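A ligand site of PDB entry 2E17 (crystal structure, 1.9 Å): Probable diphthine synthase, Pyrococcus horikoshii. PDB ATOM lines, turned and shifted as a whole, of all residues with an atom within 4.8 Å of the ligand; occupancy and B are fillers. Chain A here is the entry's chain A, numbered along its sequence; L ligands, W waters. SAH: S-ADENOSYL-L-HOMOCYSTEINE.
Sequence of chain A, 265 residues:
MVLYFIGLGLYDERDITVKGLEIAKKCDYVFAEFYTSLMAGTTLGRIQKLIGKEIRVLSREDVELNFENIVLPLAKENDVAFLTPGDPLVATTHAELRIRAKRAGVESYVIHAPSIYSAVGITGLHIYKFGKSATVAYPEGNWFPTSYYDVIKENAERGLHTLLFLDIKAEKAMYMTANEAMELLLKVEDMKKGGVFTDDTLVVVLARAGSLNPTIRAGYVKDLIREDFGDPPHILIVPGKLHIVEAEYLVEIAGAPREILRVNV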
ATOM      1  N   LEU A  10      12.971  26.786 -12.299  1.00  0.00           N
ATOM      2  CA  LEU A  10      13.074  25.841 -13.407  1.00  0.00           C
ATOM      3  C   LEU A  10      12.782  24.358 -13.299  1.00  0.00           C
ATOM      4  O   LEU A  10      12.165  23.783 -14.187  1.00  0.00           O
ATOM      5  CB  LEU A  10      14.481  25.947 -13.988  1.00  0.00           C
ATOM      6  CG  LEU A  10      15.041  27.308 -14.368  1.00  0.00           C
ATOM      7  CD1 LEU A  10      16.553  27.218 -14.467  1.00  0.00           C
ATOM      8  CD2 LEU A  10      14.428  27.792 -15.664  1.00  0.00           C
ATOM      9  N   TYR A  11      13.227  23.716 -12.224  1.00  0.00           N
ATOM     10  CA  TYR A  11      13.106  22.268 -12.152  1.00  0.00           C
ATOM     11  C   TYR A  11      12.519  21.640 -10.886  1.00  0.00           C
ATOM     12  O   TYR A  11      11.641  20.779 -10.979  1.00  0.00           O
ATOM     13  CB  TYR A  11      14.501  21.703 -12.436  1.00  0.00           C
ATOM     14  CG  TYR A  11      14.599  20.190 -12.500  1.00  0.00           C
ATOM     15  CD1 TYR A  11      14.056  19.476 -13.566  1.00  0.00           C
ATOM     16  CD2 TYR A  11      15.272  19.490 -11.503  1.00  0.00           C
ATOM     17  CE1 TYR A  11      14.189  18.090 -13.644  1.00  0.00           C
ATOM     18  CE2 TYR A  11      15.406  18.100 -11.573  1.00  0.00           C
ATOM     19  CZ  TYR A  11      14.867  17.409 -12.639  1.00  0.00           C
ATOM     20  OH  TYR A  11      15.021  16.041 -12.703  1.00  0.00           O
ATOM     21  N   THR A  36       1.497  26.692 -16.971  1.00  0.00           N
ATOM     22  CA  THR A  36       2.347  27.503 -17.843  1.00  0.00           C
ATOM     23  C   THR A  36       3.681  26.832 -18.143  1.00  0.00           C
ATOM     24  O   THR A  36       4.331  27.143 -19.141  1.00  0.00           O
ATOM     25  CB  THR A  36       2.621  28.907 -17.249  1.00  0.00           C
ATOM     26  OG1 THR A  36       3.182  28.769 -15.931  1.00  0.00           O
ATOM     27  CG2 THR A  36       1.338  29.711 -17.176  1.00  0.00           C
ATOM     28  N   SER A  37       4.091  25.912 -17.278  1.00  0.00           N
ATOM     29  CA  SER A  37       5.342  25.212 -17.509  1.00  0.00           C
ATOM     30  C   SER A  37       5.407  23.931 -16.703  1.00  0.00           C
ATOM     31  O   SER A  37       4.545  23.668 -15.868  1.00  0.00           O
ATOM     32  CB  SER A  37       6.529  26.116 -17.151  1.00  0.00           C
ATOM     33  OG  SER A  37       7.741  25.503 -17.558  1.00  0.00           O
ATOM     34  N   LEU A  38       6.431  23.129 -16.963  1.00  0.00           N
ATOM     35  CA  LEU A  38       6.617  21.865 -16.260  1.00  0.00           C
ATOM     36  C   LEU A  38       7.855  21.836 -15.391  1.00  0.00           C
ATOM     37  O   LEU A  38       8.969  22.052 -15.859  1.00  0.00           O
ATOM     38  CB  LEU A  38       6.693  20.708 -17.271  1.00  0.00           C
ATOM     39  CG  LEU A  38       7.041  19.324 -16.708  1.00  0.00           C
ATOM     40  CD1 LEU A  38       5.920  18.843 -15.792  1.00  0.00           C
ATOM     41  CD2 LEU A  38       7.245  18.339 -17.852  1.00  0.00           C
ATOM     42  N   PRO A  85       5.571  28.238 -11.987  1.00  0.00           N
ATOM     43  CA  PRO A  85       6.851  27.659 -12.391  1.00  0.00           C
ATOM     44  C   PRO A  85       7.710  28.778 -12.968  1.00  0.00           C
ATOM     45  O   PRO A  85       7.182  29.805 -13.407  1.00  0.00           O
ATOM     46  CB  PRO A  85       6.442  26.647 -13.472  1.00  0.00           C
ATOM     47  CG  PRO A  85       5.044  26.268 -13.074  1.00  0.00           C
ATOM     48  CD  PRO A  85       4.446  27.601 -12.691  1.00  0.00           C
ATOM     49  N   GLY A  86       9.031  28.584 -12.969  1.00  0.00           N
ATOM     50  CA  GLY A  86       9.936  29.593 -13.504  1.00  0.00           C
ATOM     51  C   GLY A  86       9.698  30.962 -12.902  1.00  0.00           C
ATOM     52  O   GLY A  86       9.505  31.085 -11.686  1.00  0.00           O
ATOM     53  N   ASP A  87       9.744  32.011 -13.733  1.00  0.00           N
ATOM     54  CA  ASP A  87       9.488  33.374 -13.287  1.00  0.00           C
ATOM     55  C   ASP A  87       8.018  33.611 -13.630  1.00  0.00           C
ATOM     56  O   ASP A  87       7.577  33.317 -14.744  1.00  0.00           O
ATOM     57  CB  ASP A  87      10.383  34.369 -14.027  1.00  0.00           C
ATOM     58  CG  ASP A  87      10.138  35.808 -13.592  1.00  0.00           C
ATOM     59  OD1 ASP A  87       9.029  36.336 -13.877  1.00  0.00           O
ATOM     60  OD2 ASP A  87      11.046  36.422 -12.983  1.00  0.00           O
ATOM     61  N   VAL A  90       7.233  35.696 -17.047  1.00  0.00           N
ATOM     62  CA  VAL A  90       7.919  35.383 -18.294  1.00  0.00           C
ATOM     63  C   VAL A  90       7.157  34.374 -19.143  1.00  0.00           C
ATOM     64  O   VAL A  90       6.906  33.256 -18.708  1.00  0.00           O
ATOM     65  CB  VAL A  90       9.337  34.828 -18.031  1.00  0.00           C
ATOM     66  CG1 VAL A  90       9.973  34.384 -19.339  1.00  0.00           C
ATOM     67  CG2 VAL A  90      10.198  35.896 -17.362  1.00  0.00           C
ATOM     68  N   ALA A  91       6.795  34.772 -20.356  1.00  0.00           N
ATOM     69  CA  ALA A  91       6.083  33.890 -21.268  1.00  0.00           C
ATOM     70  C   ALA A  91       4.754  33.409 -20.694  1.00  0.00           C
ATOM     71  O   ALA A  91       4.305  32.295 -20.979  1.00  0.00           O
ATOM     72  CB  ALA A  91       6.960  32.686 -21.641  1.00  0.00           C
ATOM     73  N   THR A  92       4.148  34.245 -19.869  1.00  0.00           N
ATOM     74  CA  THR A  92       2.826  34.044 -19.325  1.00  0.00           C
ATOM     75  C   THR A  92       2.034  35.324 -19.522  1.00  0.00           C
ATOM     76  O   THR A  92       2.549  36.351 -19.946  1.00  0.00           O
ATOM     77  CB  THR A  92       2.936  33.721 -17.821  1.00  0.00           C
ATOM     78  OG1 THR A  92       3.179  34.932 -17.087  1.00  0.00           O
ATOM     79  CG2 THR A  92       4.090  32.741 -17.550  1.00  0.00           C
ATOM     80  N   PRO A 114      14.522  31.696 -11.198  1.00  0.00           N
ATOM     81  CA  PRO A 114      15.228  31.346 -12.431  1.00  0.00           C
ATOM     82  C   PRO A 114      14.223  31.084 -13.552  1.00  0.00           C
ATOM     83  O   PRO A 114      13.216  30.418 -13.343  1.00  0.00           O
ATOM     84  CB  PRO A 114      15.991  30.081 -12.053  1.00  0.00           C
ATOM     85  CG  PRO A 114      16.214  30.223 -10.591  1.00  0.00           C
ATOM     86  CD  PRO A 114      14.917  30.800 -10.085  1.00  0.00           C
ATOM     87  N   SER A 115      14.523  31.629 -14.727  1.00  0.00           N
ATOM     88  CA  SER A 115      13.648  31.483 -15.897  1.00  0.00           C
ATOM     89  C   SER A 115      14.381  30.853 -17.062  1.00  0.00           C
ATOM     90  O   SER A 115      15.571  31.085 -17.257  1.00  0.00           O
ATOM     91  CB  SER A 115      13.137  32.867 -16.330  1.00  0.00           C
ATOM     92  OG  SER A 115      12.488  32.791 -17.586  1.00  0.00           O
ATOM     93  N   ILE A 116      13.683  30.047 -17.852  1.00  0.00           N
ATOM     94  CA  ILE A 116      14.304  29.404 -19.004  1.00  0.00           C
ATOM     95  C   ILE A 116      14.819  30.478 -19.963  1.00  0.00           C
ATOM     96  O   ILE A 116      15.801  30.277 -20.676  1.00  0.00           O
ATOM     97  CB  ILE A 116      13.294  28.493 -19.742  1.00  0.00           C
ATOM     98  CG1 ILE A 116      14.021  27.692 -20.828  1.00  0.00           C
ATOM     99  CG2 ILE A 116      12.197  29.347 -20.370  1.00  0.00           C
ATOM    100  CD1 ILE A 116      15.045  26.707 -20.281  1.00  0.00           C
ATOM    101  N   TYR A 117      14.165  31.642 -19.960  1.00  0.00           N
ATOM    102  CA  TYR A 117      14.558  32.736 -20.844  1.00  0.00           C
ATOM    103  C   TYR A 117      16.023  33.158 -20.656  1.00  0.00           C
ATOM    104  O   TYR A 117      16.692  33.538 -21.615  1.00  0.00           O
ATOM    105  CB  TYR A 117      13.625  33.927 -20.634  1.00  0.00           C
ATOM    106  CG  TYR A 117      13.859  35.097 -21.566  1.00  0.00           C
ATOM    107  CD1 TYR A 117      13.638  34.983 -22.938  1.00  0.00           C
ATOM    108  CD2 TYR A 117      14.271  36.333 -21.063  1.00  0.00           C
ATOM    109  CE1 TYR A 117      13.804  36.081 -23.791  1.00  0.00           C
ATOM    110  CE2 TYR A 117      14.445  37.433 -21.905  1.00  0.00           C
ATOM    111  CZ  TYR A 117      14.214  37.297 -23.263  1.00  0.00           C
ATOM    112  OH  TYR A 117      14.372  38.389 -24.072  1.00  0.00           O
ATOM    113  N   PHE A 165      10.068  28.533 -27.371  1.00  0.00           N
ATOM    114  CA  PHE A 165       9.375  27.910 -26.262  1.00  0.00           C
ATOM    115  C   PHE A 165       8.559  26.818 -26.940  1.00  0.00           C
ATOM    116  O   PHE A 165       8.074  27.021 -28.053  1.00  0.00           O
ATOM    117  CB  PHE A 165       8.421  28.905 -25.603  1.00  0.00           C
ATOM    118  CG  PHE A 165       9.097  30.052 -24.910  1.00  0.00           C
ATOM    119  CD1 PHE A 165       9.618  29.894 -23.637  1.00  0.00           C
ATOM    120  CD2 PHE A 165       9.203  31.288 -25.532  1.00  0.00           C
ATOM    121  CE1 PHE A 165      10.248  30.955 -22.985  1.00  0.00           C
ATOM    122  CE2 PHE A 165       9.830  32.358 -24.898  1.00  0.00           C
ATOM    123  CZ  PHE A 165      10.353  32.196 -23.617  1.00  0.00           C
ATOM    124  N   LEU A 166       8.418  25.659 -26.286  1.00  0.00           N
ATOM    125  CA  LEU A 166       7.651  24.562 -26.864  1.00  0.00           C
ATOM    126  C   LEU A 166       6.287  24.440 -26.175  1.00  0.00           C
ATOM    127  O   LEU A 166       6.150  24.726 -24.984  1.00  0.00           O
ATOM    128  CB  LEU A 166       8.449  23.261 -26.755  1.00  0.00           C
ATOM    129  CG  LEU A 166       9.830  23.332 -27.414  1.00  0.00           C
ATOM    130  CD1 LEU A 166      10.453  21.947 -27.468  1.00  0.00           C
ATOM    131  CD2 LEU A 166       9.700  23.909 -28.831  1.00  0.00           C
ATOM    132  N   ASP A 167       5.289  24.011 -26.940  1.00  0.00           N
ATOM    133  CA  ASP A 167       3.916  23.896 -26.436  1.00  0.00           C
ATOM    134  C   ASP A 167       3.728  22.967 -25.245  1.00  0.00           C
ATOM    135  O   ASP A 167       4.504  22.052 -25.012  1.00  0.00           O
ATOM    136  CB  ASP A 167       2.992  23.469 -27.581  1.00  0.00           C
ATOM    137  CG  ASP A 167       1.576  24.022 -27.421  1.00  0.00           C
ATOM    138  OD1 ASP A 167       1.304  24.674 -26.394  1.00  0.00           O
ATOM    139  OD2 ASP A 167       0.743  23.803 -28.330  1.00  0.00           O
ATOM    140  N   ILE A 168       2.678  23.245 -24.486  1.00  0.00           N
ATOM    141  CA  ILE A 168       2.337  22.446 -23.309  1.00  0.00           C
ATOM    142  C   ILE A 168       0.828  22.390 -23.099  1.00  0.00           C
ATOM    143  O   ILE A 168       0.141  23.409 -23.156  1.00  0.00           O
ATOM    144  CB  ILE A 168       3.010  23.008 -22.035  1.00  0.00           C
ATOM    145  CG1 ILE A 168       2.491  22.260 -20.803  1.00  0.00           C
ATOM    146  CG2 ILE A 168       2.727  24.505 -21.912  1.00  0.00           C
ATOM    147  CD1 ILE A 168       3.100  22.730 -19.493  1.00  0.00           C
ATOM    148  N   LEU A 206      17.969  22.164 -25.199  1.00  0.00           N
ATOM    149  CA  LEU A 206      18.230  22.252 -23.768  1.00  0.00           C
ATOM    150  C   LEU A 206      17.035  21.593 -23.098  1.00  0.00           C
ATOM    151  O   LEU A 206      15.899  22.052 -23.254  1.00  0.00           O
ATOM    152  CB  LEU A 206      18.353  23.707 -23.302  1.00  0.00           C
ATOM    153  CG  LEU A 206      18.510  23.907 -21.790  1.00  0.00           C
ATOM    154  CD1 LEU A 206      19.724  23.136 -21.290  1.00  0.00           C
ATOM    155  CD2 LEU A 206      18.653  25.399 -21.467  1.00  0.00           C
ATOM    156  N   ALA A 207      17.282  20.514 -22.366  1.00  0.00           N
ATOM    157  CA  ALA A 207      16.199  19.811 -21.704  1.00  0.00           C
ATOM    158  C   ALA A 207      16.403  19.779 -20.207  1.00  0.00           C
ATOM    159  O   ALA A 207      17.500  19.504 -19.714  1.00  0.00           O
ATOM    160  CB  ALA A 207      16.091  18.392 -22.245  1.00  0.00           C
ATOM    161  N   ARG A 208      15.332  20.071 -19.481  1.00  0.00           N
ATOM    162  CA  ARG A 208      15.341  20.076 -18.021  1.00  0.00           C
ATOM    163  C   ARG A 208      16.379  21.018 -17.429  1.00  0.00           C
ATOM    164  O   ARG A 208      17.164  20.638 -16.551  1.00  0.00           O
ATOM    165  CB  ARG A 208      15.567  18.636 -17.506  1.00  0.00           C
ATOM    166  CG  ARG A 208      14.523  17.635 -18.023  1.00  0.00           C
ATOM    167  CD  ARG A 208      14.816  16.224 -17.529  1.00  0.00           C
ATOM    168  NE  ARG A 208      16.189  15.833 -17.819  1.00  0.00           N
ATOM    169  CZ  ARG A 208      16.668  15.602 -19.035  1.00  0.00           C
ATOM    170  NH1 ARG A 208      15.891  15.712 -20.105  1.00  0.00           N
ATOM    171  NH2 ARG A 208      17.950  15.281 -19.187  1.00  0.00           N
ATOM    172  N   ALA A 209      16.380  22.257 -17.921  1.00  0.00           N
ATOM    173  CA  ALA A 209      17.296  23.260 -17.391  1.00  0.00           C
ATOM    174  C   ALA A 209      16.921  23.374 -15.913  1.00  0.00           C
ATOM    175  O   ALA A 209      15.751  23.202 -15.560  1.00  0.00           O
ATOM    176  CB  ALA A 209      17.073  24.597 -18.087  1.00  0.00           C
ATOM    177  N   GLY A 210      17.891  23.649 -15.057  1.00  0.00           N
ATOM    178  CA  GLY A 210      17.581  23.750 -13.642  1.00  0.00           C
ATOM    179  C   GLY A 210      18.042  22.514 -12.897  1.00  0.00           C
ATOM    180  O   GLY A 210      18.397  22.576 -11.717  1.00  0.00           O
ATOM    181  N   PRO A 233      10.652  19.186 -19.475  1.00  0.00           N
ATOM    182  CA  PRO A 233      10.413  20.083 -20.604  1.00  0.00           C
ATOM    183  C   PRO A 233      11.657  20.299 -21.473  1.00  0.00           C
ATOM    184  O   PRO A 233      12.792  20.154 -21.018  1.00  0.00           O
ATOM    185  CB  PRO A 233       9.959  21.365 -19.926  1.00  0.00           C
ATOM    186  CG  PRO A 233      10.818  21.395 -18.695  1.00  0.00           C
ATOM    187  CD  PRO A 233      10.762  19.946 -18.212  1.00  0.00           C
ATOM    188  N   HIS A 234      11.416  20.653 -22.728  1.00  0.00           N
ATOM    189  CA  HIS A 234      12.471  20.907 -23.702  1.00  0.00           C
ATOM    190  C   HIS A 234      12.305  22.300 -24.294  1.00  0.00           C
ATOM    191  O   HIS A 234      11.201  22.840 -24.352  1.00  0.00           O
ATOM    192  CB  HIS A 234      12.395  19.928 -24.894  1.00  0.00           C
ATOM    193  CG  HIS A 234      12.664  18.500 -24.549  1.00  0.00           C
ATOM    194  ND1 HIS A 234      12.664  17.504 -25.495  1.00  0.00           N
ATOM    195  CD2 HIS A 234      12.946  17.895 -23.372  1.00  0.00           C
ATOM    196  CE1 HIS A 234      12.943  16.347 -24.926  1.00  0.00           C
ATOM    197  NE2 HIS A 234      13.122  16.553 -23.639  1.00  0.00           N
ATOM    198  N   ILE A 235      13.423  22.868 -24.746  1.00  0.00           N
ATOM    199  CA  ILE A 235      13.389  24.161 -25.407  1.00  0.00           C
ATOM    200  C   ILE A 235      14.256  23.957 -26.647  1.00  0.00           C
ATOM    201  O   ILE A 235      15.220  23.179 -26.617  1.00  0.00           O
ATOM    202  CB  ILE A 235      13.985  25.278 -24.511  1.00  0.00           C
ATOM    203  CG1 ILE A 235      13.530  26.638 -25.034  1.00  0.00           C
ATOM    204  CG2 ILE A 235      15.495  25.210 -24.489  1.00  0.00           C
ATOM    205  CD1 ILE A 235      12.319  27.177 -24.337  1.00  0.00           C
HETATM  206  N   SAH L   1       7.544  31.493 -16.865  1.00  0.00           N
HETATM  207  CA  SAH L   1       8.325  30.293 -17.375  1.00  0.00           C
HETATM  208  CB  SAH L   1       8.149  29.908 -18.813  1.00  0.00           C
HETATM  209  CG  SAH L   1       6.751  29.603 -19.327  1.00  0.00           C
HETATM  210  SD  SAH L   1       6.947  28.944 -21.034  1.00  0.00           S
HETATM  211  C   SAH L   1       9.851  30.580 -17.059  1.00  0.00           C
HETATM  212  O   SAH L   1      10.158  31.662 -16.507  1.00  0.00           O
HETATM  213  OXT SAH L   1      10.693  29.662 -17.395  1.00  0.00           O
HETATM  214  C5' SAH L   1       6.931  27.210 -20.788  1.00  0.00           C
HETATM  215  C4' SAH L   1       7.912  26.540 -21.838  1.00  0.00           C
HETATM  216  O4' SAH L   1       9.263  27.035 -21.585  1.00  0.00           O
HETATM  217  C3' SAH L   1       7.994  25.052 -21.787  1.00  0.00           C
HETATM  218  O3' SAH L   1       6.950  24.456 -22.553  1.00  0.00           O
HETATM  219  C2' SAH L   1       9.431  24.794 -22.306  1.00  0.00           C
HETATM  220  O2' SAH L   1       9.531  24.751 -23.737  1.00  0.00           O
HETATM  221  C1' SAH L   1      10.280  25.909 -21.624  1.00  0.00           C
HETATM  222  N9  SAH L   1      10.784  25.610 -20.336  1.00  0.00           N
HETATM  223  C8  SAH L   1      10.414  25.969 -19.047  1.00  0.00           C
HETATM  224  N7  SAH L   1      11.149  25.476 -18.100  1.00  0.00           N
HETATM  225  C5  SAH L   1      12.133  24.695 -18.778  1.00  0.00           C
HETATM  226  C6  SAH L   1      13.234  23.906 -18.288  1.00  0.00           C
HETATM  227  N6  SAH L   1      13.529  23.751 -16.985  1.00  0.00           N
HETATM  228  N1  SAH L   1      13.982  23.288 -19.261  1.00  0.00           N
HETATM  229  C2  SAH L   1      13.723  23.406 -20.598  1.00  0.00           C
HETATM  230  N3  SAH L   1      12.677  24.148 -21.097  1.00  0.00           N
HETATM  231  C4  SAH L   1      11.935  24.765 -20.137  1.00  0.00           C
HETATM  232  O   HOH W   1       5.669  29.730 -15.845  1.00  0.00           O
HETATM  233  O   HOH W   2       6.346  21.706 -22.635  1.00  0.00           O
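An oxygen (O2') of the ligand is in hydrogen-bond range of the backbone carbonyl oxygen of His 234 (2.6 Å). N of Ala 209 is in hydrogen-bond range of N1 of the ligand (2.9 Å). N of Asp 87 lies within hydrogen-bond range of O of the ligand. A nitrogen (N) of the ligand lies within hydrogen-bond range of the backbone carbonyl oxygen of Asp 87, 2.8 Å away. An oxygen (O3') of the ligand is in hydrogen-bond range of the backbone carbonyl oxygen (O) of Leu 166 (2.6 Å). The backbone NH of Arg 208 sits at hydrogen-bond distance from a nitrogen (N1) of the ligand (3.5 Å). The backbone NH (N) of Ile 116 is in hydrogen-bond range of an oxygen (OXT) of the ligand (3.0 Å). The side-chain hydroxyl (OG) of Ser 115 lies within hydrogen-bond range of an oxygen (O) of the ligand, 2.8 Å away. A nitrogen (N) of the ligand sits at hydrogen-bond distance from the backbone carbonyl oxygen (O) of Val 90 (2.6 Å). N of Leu 166 lies within hydrogen-bond range of O2' of the ligand (2.9 Å). N6 of the ligand sits at hydrogen-bond distance from O of Ala 209, 2.7 Å away. A nitrogen (N7) of the ligand lies close to the side-chain hydroxyl of Ser 37 (3.5 Å). A nitrogen (N6) of the ligand is in hydrogen-bond range of the backbone carbonyl oxygen of Leu 10, at 3.1 Å.
OG of Ser 115 sits close to N of Tyr 117 (3.1 Å). N of Arg 208 sits at hydrogen-bond distance from O of Pro 233 (3.0 Å). The backbone carbonyl oxygen (O) of Leu 206 lies within hydrogen-bond range of the backbone NH (N) of Ile 235.
The backbone carbonyl oxygen (O) of Thr 36 lies close to a sulfur (SD) of the ligand, 3.7 Å away. Pro 85 touches the ligand (O to N, 3.9 Å). Gly 86 touches the ligand. CB of Ala 91 touches SD of the ligand, at 3.8 Å. Thr 92 touches the ligand. CD1 of Phe 165 touches O4' of the ligand, 3.5 Å away. Leu 206 touches the ligand (O to C2, 3.7 Å). O of Pro 233 touches C2 of the ligand, 3.4 Å away. CD1 of Ile 235 touches C1' of the ligand, at 3.6 Å. Hydrophobic or aromatic side chains that line the ligand: Leu 10, Val 90, Ala 91, Ile 116, Phe 165, Leu 166, Ala 209, Pro 233 and Ile 235. 19 residues have an atom within 4 Å of the ligand: Leu 10, Thr 36, Ser 37, Pro 85, Gly 86, Asp 87, Val 90, Ala 91, Thr 92, Ser 115, Ile 116, Phe 165, Leu 166, Leu 206, Arg 208, Ala 209, Pro 233, His 234 and Ile 235. The nearest printed residue that does not touch the ligand is Asp 167 (4.2 Å).
Water W1 lies within hydrogen-bond range of the side-chain hydroxyl (OG1) of Thr 36, a nitrogen (N) of the ligand and the backbone carbonyl oxygen (O) of Pro 85. Water W2 lies within hydrogen-bond range of O3' of the ligand (2.8 Å) and O of Asp 167 (3.0 Å).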
